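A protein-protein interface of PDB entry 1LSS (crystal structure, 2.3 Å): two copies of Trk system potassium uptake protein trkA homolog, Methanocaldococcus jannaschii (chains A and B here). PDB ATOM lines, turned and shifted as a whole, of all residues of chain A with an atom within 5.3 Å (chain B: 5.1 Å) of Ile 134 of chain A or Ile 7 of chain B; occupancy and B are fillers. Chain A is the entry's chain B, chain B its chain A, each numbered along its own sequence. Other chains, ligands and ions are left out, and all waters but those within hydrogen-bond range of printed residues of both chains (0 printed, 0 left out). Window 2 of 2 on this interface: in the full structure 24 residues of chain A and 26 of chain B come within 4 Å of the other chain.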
ATOM      1  N   ILE A 130      30.336  24.337  11.942  1.00  0.00           N
ATOM      2  CA  ILE A 130      30.765  24.952  13.193  1.00  0.00           C
ATOM      3  C   ILE A 130      30.359  24.036  14.342  1.00  0.00           C
ATOM      4  O   ILE A 130      31.117  23.825  15.288  1.00  0.00           O
ATOM      5  CB  ILE A 130      30.103  26.338  13.393  1.00  0.00           C
ATOM      6  CG1 ILE A 130      30.684  27.341  12.395  1.00  0.00           C
ATOM      7  CG2 ILE A 130      30.302  26.820  14.817  1.00  0.00           C
ATOM      8  CD1 ILE A 130      30.029  28.722  12.450  1.00  0.00           C
ATOM      9  N   GLU A 131      29.157  23.482  14.247  1.00  0.00           N
ATOM     10  CA  GLU A 131      28.668  22.585  15.274  1.00  0.00           C
ATOM     11  C   GLU A 131      29.620  21.393  15.466  1.00  0.00           C
ATOM     12  O   GLU A 131      29.839  20.936  16.593  1.00  0.00           O
ATOM     13  CB  GLU A 131      27.266  22.101  14.912  1.00  0.00           C
ATOM     14  CG  GLU A 131      26.686  21.116  15.899  1.00  0.00           C
ATOM     15  CD  GLU A 131      25.249  20.767  15.579  1.00  0.00           C
ATOM     16  OE1 GLU A 131      24.796  21.101  14.454  1.00  0.00           O
ATOM     17  OE2 GLU A 131      24.581  20.154  16.448  1.00  0.00           O
ATOM     18  N   LYS A 132      30.211  20.902  14.378  1.00  0.00           N
ATOM     19  CA  LYS A 132      31.122  19.771  14.456  1.00  0.00           C
ATOM     20  C   LYS A 132      32.422  20.171  15.137  1.00  0.00           C
ATOM     21  O   LYS A 132      33.007  19.360  15.868  1.00  0.00           O
ATOM     22  CB  LYS A 132      31.379  19.206  13.060  1.00  0.00           C
ATOM     23  CG  LYS A 132      30.127  18.693  12.366  1.00  0.00           C
ATOM     24  CD  LYS A 132      30.470  17.943  11.091  1.00  0.00           C
ATOM     25  CE  LYS A 132      29.216  17.437  10.394  1.00  0.00           C
ATOM     26  NZ  LYS A 132      29.535  16.695   9.145  1.00  0.00           N
ATOM     27  N   LEU A 133      32.901  21.388  14.907  1.00  0.00           N
ATOM     28  CA  LEU A 133      34.137  21.849  15.539  1.00  0.00           C
ATOM     29  C   LEU A 133      33.957  21.984  17.050  1.00  0.00           C
ATOM     30  O   LEU A 133      34.923  21.911  17.811  1.00  0.00           O
ATOM     31  CB  LEU A 133      34.574  23.198  14.963  1.00  0.00           C
ATOM     32  CG  LEU A 133      34.916  23.239  13.473  1.00  0.00           C
ATOM     33  CD1 LEU A 133      35.488  24.599  13.123  1.00  0.00           C
ATOM     34  CD2 LEU A 133      35.916  22.142  13.140  1.00  0.00           C
ATOM     35  N   ILE A 134      32.719  22.186  17.481  1.00  0.00           N
ATOM     36  CA  ILE A 134      32.439  22.332  18.901  1.00  0.00           C
ATOM     37  C   ILE A 134      32.380  20.973  19.579  1.00  0.00           C
ATOM     38  O   ILE A 134      32.809  20.828  20.720  1.00  0.00           O
ATOM     39  CB  ILE A 134      31.102  23.070  19.139  1.00  0.00           C
ATOM     40  CG1 ILE A 134      31.196  24.500  18.601  1.00  0.00           C
ATOM     41  CG2 ILE A 134      30.768  23.078  20.620  1.00  0.00           C
ATOM     42  CD1 ILE A 134      29.919  25.310  18.783  1.00  0.00           C
ATOM     43  N   GLU A 135      31.846  19.980  18.876  1.00  0.00           N
ATOM     44  CA  GLU A 135      31.734  18.627  19.415  1.00  0.00           C
ATOM     45  C   GLU A 135      33.107  17.955  19.354  1.00  0.00           C
ATOM     46  O   GLU A 135      33.299  16.854  19.874  1.00  0.00           O
ATOM     47  CB  GLU A 135      30.733  17.806  18.597  1.00  0.00           C
ATOM     48  CG  GLU A 135      29.393  18.488  18.284  1.00  0.00           C
ATOM     49  CD  GLU A 135      28.605  18.888  19.521  1.00  0.00           C
ATOM     50  OE1 GLU A 135      28.622  18.130  20.520  1.00  0.00           O
ATOM     51  OE2 GLU A 135      27.951  19.956  19.488  1.00  0.00           O
ATOM     52  N   ARG A 136      34.052  18.642  18.714  1.00  0.00           N
ATOM     53  CA  ARG A 136      35.422  18.161  18.533  1.00  0.00           C
ATOM     54  C   ARG A 136      35.490  16.913  17.663  1.00  0.00           C
ATOM     55  O   ARG A 136      35.708  17.004  16.451  1.00  0.00           O
ATOM     56  CB  ARG A 136      36.097  17.890  19.887  1.00  0.00           C
ATOM     57  CG  ARG A 136      36.447  19.145  20.688  1.00  0.00           C
ATOM     58  CD  ARG A 136      37.030  20.228  19.786  1.00  0.00           C
ATOM     59  NE  ARG A 136      37.706  21.293  20.525  1.00  0.00           N
ATOM     60  CZ  ARG A 136      38.938  21.194  21.019  1.00  0.00           C
ATOM     61  NH1 ARG A 136      39.640  20.076  20.854  1.00  0.00           N
ATOM     62  NH2 ARG A 136      39.480  22.221  21.664  1.00  0.00           N
ATOM     63  N   MET B   5      31.687  24.922  28.828  1.00  0.00           N
ATOM     64  CA  MET B   5      31.245  26.210  29.436  1.00  0.00           C
ATOM     65  C   MET B   5      30.236  26.945  28.537  1.00  0.00           C
ATOM     66  O   MET B   5      29.602  26.341  27.671  1.00  0.00           O
ATOM     67  CB  MET B   5      32.474  27.093  29.718  1.00  0.00           C
ATOM     68  CG  MET B   5      33.485  26.457  30.695  1.00  0.00           C
ATOM     69  SD  MET B   5      34.970  27.452  31.083  1.00  0.00           S
ATOM     70  CE  MET B   5      34.453  28.307  32.594  1.00  0.00           C
ATOM     71  N   TYR B   6      30.080  28.246  28.757  1.00  0.00           N
ATOM     72  CA  TYR B   6      29.147  29.050  27.978  1.00  0.00           C
ATOM     73  C   TYR B   6      29.615  29.331  26.550  1.00  0.00           C
ATOM     74  O   TYR B   6      30.795  29.514  26.301  1.00  0.00           O
ATOM     75  CB  TYR B   6      28.874  30.380  28.699  1.00  0.00           C
ATOM     76  CG  TYR B   6      27.738  30.326  29.702  1.00  0.00           C
ATOM     77  CD1 TYR B   6      27.788  29.472  30.807  1.00  0.00           C
ATOM     78  CD2 TYR B   6      26.592  31.110  29.525  1.00  0.00           C
ATOM     79  CE1 TYR B   6      26.720  29.393  31.711  1.00  0.00           C
ATOM     80  CE2 TYR B   6      25.518  31.043  30.419  1.00  0.00           C
ATOM     81  CZ  TYR B   6      25.588  30.181  31.510  1.00  0.00           C
ATOM     82  OH  TYR B   6      24.525  30.090  32.385  1.00  0.00           O
ATOM     83  N   ILE B   7      28.662  29.360  25.623  1.00  0.00           N
ATOM     84  CA  ILE B   7      28.917  29.643  24.212  1.00  0.00           C
ATOM     85  C   ILE B   7      28.126  30.889  23.791  1.00  0.00           C
ATOM     86  O   ILE B   7      26.890  30.917  23.868  1.00  0.00           O
ATOM     87  CB  ILE B   7      28.485  28.466  23.310  1.00  0.00           C
ATOM     88  CG1 ILE B   7      29.427  27.277  23.505  1.00  0.00           C
ATOM     89  CG2 ILE B   7      28.489  28.904  21.853  1.00  0.00           C
ATOM     90  CD1 ILE B   7      29.051  26.037  22.676  1.00  0.00           C
ATOM     91  N   ILE B   8      28.842  31.920  23.356  1.00  0.00           N
ATOM     92  CA  ILE B   8      28.210  33.157  22.921  1.00  0.00           C
ATOM     93  C   ILE B   8      28.139  33.172  21.398  1.00  0.00           C
ATOM     94  O   ILE B   8      29.129  32.879  20.724  1.00  0.00           O
ATOM     95  CB  ILE B   8      29.013  34.385  23.405  1.00  0.00           C
ATOM     96  CG1 ILE B   8      29.014  34.427  24.939  1.00  0.00           C
ATOM     97  CG2 ILE B   8      28.420  35.673  22.815  1.00  0.00           C
ATOM     98  CD1 ILE B   8      29.972  35.443  25.532  1.00  0.00           C
ATOM     99  N   ILE B   9      26.963  33.505  20.865  1.00  0.00           N
ATOM    100  CA  ILE B   9      26.744  33.563  19.416  1.00  0.00           C
ATOM    101  C   ILE B   9      26.216  34.937  19.044  1.00  0.00           C
ATOM    102  O   ILE B   9      25.188  35.368  19.575  1.00  0.00           O
ATOM    103  CB  ILE B   9      25.700  32.520  18.950  1.00  0.00           C
ATOM    104  CG1 ILE B   9      26.176  31.115  19.309  1.00  0.00           C
ATOM    105  CG2 ILE B   9      25.451  32.655  17.452  1.00  0.00           C
ATOM    106  CD1 ILE B   9      25.140  30.046  19.047  1.00  0.00           C
ATOM    107  N   LEU B  19      22.459  27.403  14.243  1.00  0.00           N
ATOM    108  CA  LEU B  19      23.474  26.962  15.178  1.00  0.00           C
ATOM    109  C   LEU B  19      22.909  27.052  16.598  1.00  0.00           C
ATOM    110  O   LEU B  19      23.056  26.123  17.395  1.00  0.00           O
ATOM    111  CB  LEU B  19      24.714  27.838  15.044  1.00  0.00           C
ATOM    112  CG  LEU B  19      25.918  27.521  15.931  1.00  0.00           C
ATOM    113  CD1 LEU B  19      26.400  26.082  15.687  1.00  0.00           C
ATOM    114  CD2 LEU B  19      27.010  28.535  15.625  1.00  0.00           C
ATOM    115  N   LEU B  23      22.685  23.744  18.905  1.00  0.00           N
ATOM    116  CA  LEU B  23      23.544  23.661  20.087  1.00  0.00           C
ATOM    117  C   LEU B  23      22.769  23.532  21.391  1.00  0.00           C
ATOM    118  O   LEU B  23      23.148  22.739  22.247  1.00  0.00           O
ATOM    119  CB  LEU B  23      24.484  24.871  20.190  1.00  0.00           C
ATOM    120  CG  LEU B  23      25.684  24.914  19.241  1.00  0.00           C
ATOM    121  CD1 LEU B  23      26.515  26.169  19.526  1.00  0.00           C
ATOM    122  CD2 LEU B  23      26.529  23.650  19.409  1.00  0.00           C
ATOM    123  N   HIS B  28      23.940  22.411  25.479  1.00  0.00           N
ATOM    124  CA  HIS B  28      24.854  23.538  25.643  1.00  0.00           C
ATOM    125  C   HIS B  28      24.235  24.801  26.235  1.00  0.00           C
ATOM    126  O   HIS B  28      23.052  25.074  26.043  1.00  0.00           O
ATOM    127  CB  HIS B  28      25.479  23.897  24.296  1.00  0.00           C
ATOM    128  CG  HIS B  28      26.458  22.887  23.795  1.00  0.00           C
ATOM    129  ND1 HIS B  28      27.736  22.781  24.296  1.00  0.00           N
ATOM    130  CD2 HIS B  28      26.346  21.940  22.834  1.00  0.00           C
ATOM    131  CE1 HIS B  28      28.374  21.812  23.660  1.00  0.00           C
ATOM    132  NE2 HIS B  28      27.552  21.288  22.769  1.00  0.00           N
ATOM    133  N   ASP B  29      25.049  25.571  26.951  1.00  0.00           N
ATOM    134  CA  ASP B  29      24.609  26.835  27.546  1.00  0.00           C
ATOM    135  C   ASP B  29      24.987  27.932  26.562  1.00  0.00           C
ATOM    136  O   ASP B  29      26.169  28.210  26.359  1.00  0.00           O
ATOM    137  CB  ASP B  29      25.333  27.101  28.869  1.00  0.00           C
ATOM    138  CG  ASP B  29      24.759  26.316  30.025  1.00  0.00           C
ATOM    139  OD1 ASP B  29      24.839  25.070  30.011  1.00  0.00           O
ATOM    140  OD2 ASP B  29      24.224  26.957  30.952  1.00  0.00           O
ATOM    141  N   ILE B  30      23.999  28.569  25.953  1.00  0.00           N
ATOM    142  CA  ILE B  30      24.322  29.599  24.988  1.00  0.00           C
ATOM    143  C   ILE B  30      23.642  30.940  25.218  1.00  0.00           C
ATOM    144  O   ILE B  30      22.566  31.030  25.811  1.00  0.00           O
ATOM    145  CB  ILE B  30      23.998  29.113  23.556  1.00  0.00           C
ATOM    146  CG1 ILE B  30      22.487  29.108  23.336  1.00  0.00           C
ATOM    147  CG2 ILE B  30      24.514  27.679  23.356  1.00  0.00           C
ATOM    148  CD1 ILE B  30      22.077  28.706  21.934  1.00  0.00           C
ATOM    149  N   VAL B  31      24.301  31.990  24.754  1.00  0.00           N
ATOM    150  CA  VAL B  31      23.744  33.323  24.857  1.00  0.00           C
ATOM    151  C   VAL B  31      23.857  33.918  23.460  1.00  0.00           C
ATOM    152  O   VAL B  31      24.878  33.779  22.797  1.00  0.00           O
ATOM    153  CB  VAL B  31      24.483  34.179  25.949  1.00  0.00           C
ATOM    154  CG1 VAL B  31      25.937  33.766  26.057  1.00  0.00           C
ATOM    155  CG2 VAL B  31      24.359  35.659  25.631  1.00  0.00           C
ATOM    156  N   ASP B  71      33.328  30.256  27.047  1.00  0.00           N
ATOM    157  CA  ASP B  71      34.337  29.305  26.615  1.00  0.00           C
ATOM    158  C   ASP B  71      34.509  29.422  25.112  1.00  0.00           C
ATOM    159  O   ASP B  71      35.532  29.028  24.557  1.00  0.00           O
ATOM    160  CB  ASP B  71      33.920  27.880  26.967  1.00  0.00           C
ATOM    161  CG  ASP B  71      34.943  26.850  26.521  1.00  0.00           C
ATOM    162  OD1 ASP B  71      36.117  26.964  26.946  1.00  0.00           O
ATOM    163  OD2 ASP B  71      34.579  25.933  25.748  1.00  0.00           O
ATOM    164  N   MET B  72      33.505  29.990  24.450  1.00  0.00           N
ATOM    165  CA  MET B  72      33.559  30.123  23.006  1.00  0.00           C
ATOM    166  C   MET B  72      32.806  31.359  22.549  1.00  0.00           C
ATOM    167  O   MET B  72      31.789  31.725  23.133  1.00  0.00           O
ATOM    168  CB  MET B  72      32.942  28.876  22.390  1.00  0.00           C
ATOM    169  CG  MET B  72      33.373  28.539  20.997  1.00  0.00           C
ATOM    170  SD  MET B  72      32.820  26.851  20.639  1.00  0.00           S
ATOM    171  CE  MET B  72      33.687  25.939  21.960  1.00  0.00           C
ATOM    172  N   ILE B  74      31.314  33.019  18.957  1.00  0.00           N
ATOM    173  CA  ILE B  74      31.009  32.795  17.544  1.00  0.00           C
ATOM    174  C   ILE B  74      30.306  33.986  16.898  1.00  0.00           C
ATOM    175  O   ILE B  74      29.143  34.275  17.199  1.00  0.00           O
ATOM    176  CB  ILE B  74      30.127  31.536  17.399  1.00  0.00           C
ATOM    177  CG1 ILE B  74      30.851  30.338  18.025  1.00  0.00           C
ATOM    178  CG2 ILE B  74      29.798  31.279  15.930  1.00  0.00           C
ATOM    179  CD1 ILE B  74      30.058  29.046  17.995  1.00  0.00           C
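N of Met 72 of chain B is in hydrogen-bond range of O of Tyr 6 of chain B (3.3 Å). The backbone NH (N) of Ile 74 of chain B sits at hydrogen-bond distance from the backbone carbonyl oxygen (O) of Ile 8 of chain B (2.8 Å). O of Ile 7 of chain B lies within hydrogen-bond range of N of Val 31 of chain B, 2.9 Å away. The backbone NH (N) of His 28 of chain B lies close to the backbone carbonyl oxygen (O) of Leu 23 of chain B, 3.3 Å away. The backbone NH (N) of Ile 8 of chain B lies within hydrogen-bond range of the backbone carbonyl oxygen (O) of Met 72 of chain B (3.0 Å). N of Ile 7 of chain B lies within hydrogen-bond range of O of Asp 29 of chain B (2.8 Å).
Among the printed residues, pairs that only touch across the chains: Ile 134 of chain A with Met 72 of chain B, Glu 135 of chain A with His 28 of chain B, Ile 134 of chain A with Leu 23 of chain B, Ile 130 of chain A with Leu 19 of chain B, Ile 134 of chain A with Ile 74 of chain B, Ile 130 of chain A with Ile 74 of chain B, Glu 135 of chain A with Leu 23 of chain B and Ile 134 of chain A with Ile 7 of chain B.
Of the printed residues of chain B, Ile 134 of chain A touches Ile 7 (3.99 Å), Leu 23 (3.6 Å), Met 72 (3.5 Å) and Ile 74 (3.8 Å). Printed residues of chain A within 4 Å of Ile 7 of chain B: Ile 134. Printed residues of chain A within 4 Å of Leu 19 of chain B: Ile 130. Of the printed residues of chain B, Ile 130 of chain A touches Leu 19 and Ile 74. Of the printed residues of chain A, Leu 23 of chain B touches Ile 134 (3.6 Å) and Glu 135 (3.96 Å). Printed residues of chain A within 4 Å of His 28 of chain B: Glu 135 (3.6 Å). Asp 71 of chain B touches none of the printed residues of chain A. Leu 133 of chain A touches none of the printed residues of chain B. The nearest printed residue of chain B that does not touch Ile 134 of chain A is His 28 of chain B (4.1 Å).
Of the 14 printed residues of chain B, 6 touch a printed residue of chain A. Of the 7 printed residues of chain A, 3 touch a printed residue of chain B. Printed residues of chain A that touch a printed residue of chain B: Ile 130, Ile 134 and Glu 135. Hydrophobic or aromatic side chains of chain A within 4 Å of the printed part of chain B: Ile 130 and Ile 134. Along chain A the printed residues that touch a printed residue of chain B span positions 130 to 135. Among the printed residues, 8 pairs touch across the chains.
No position is printed for both chains. Of the 8 pairs that touch across the chains among the printed residues, none has its exchanged pair printed and touching as well.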
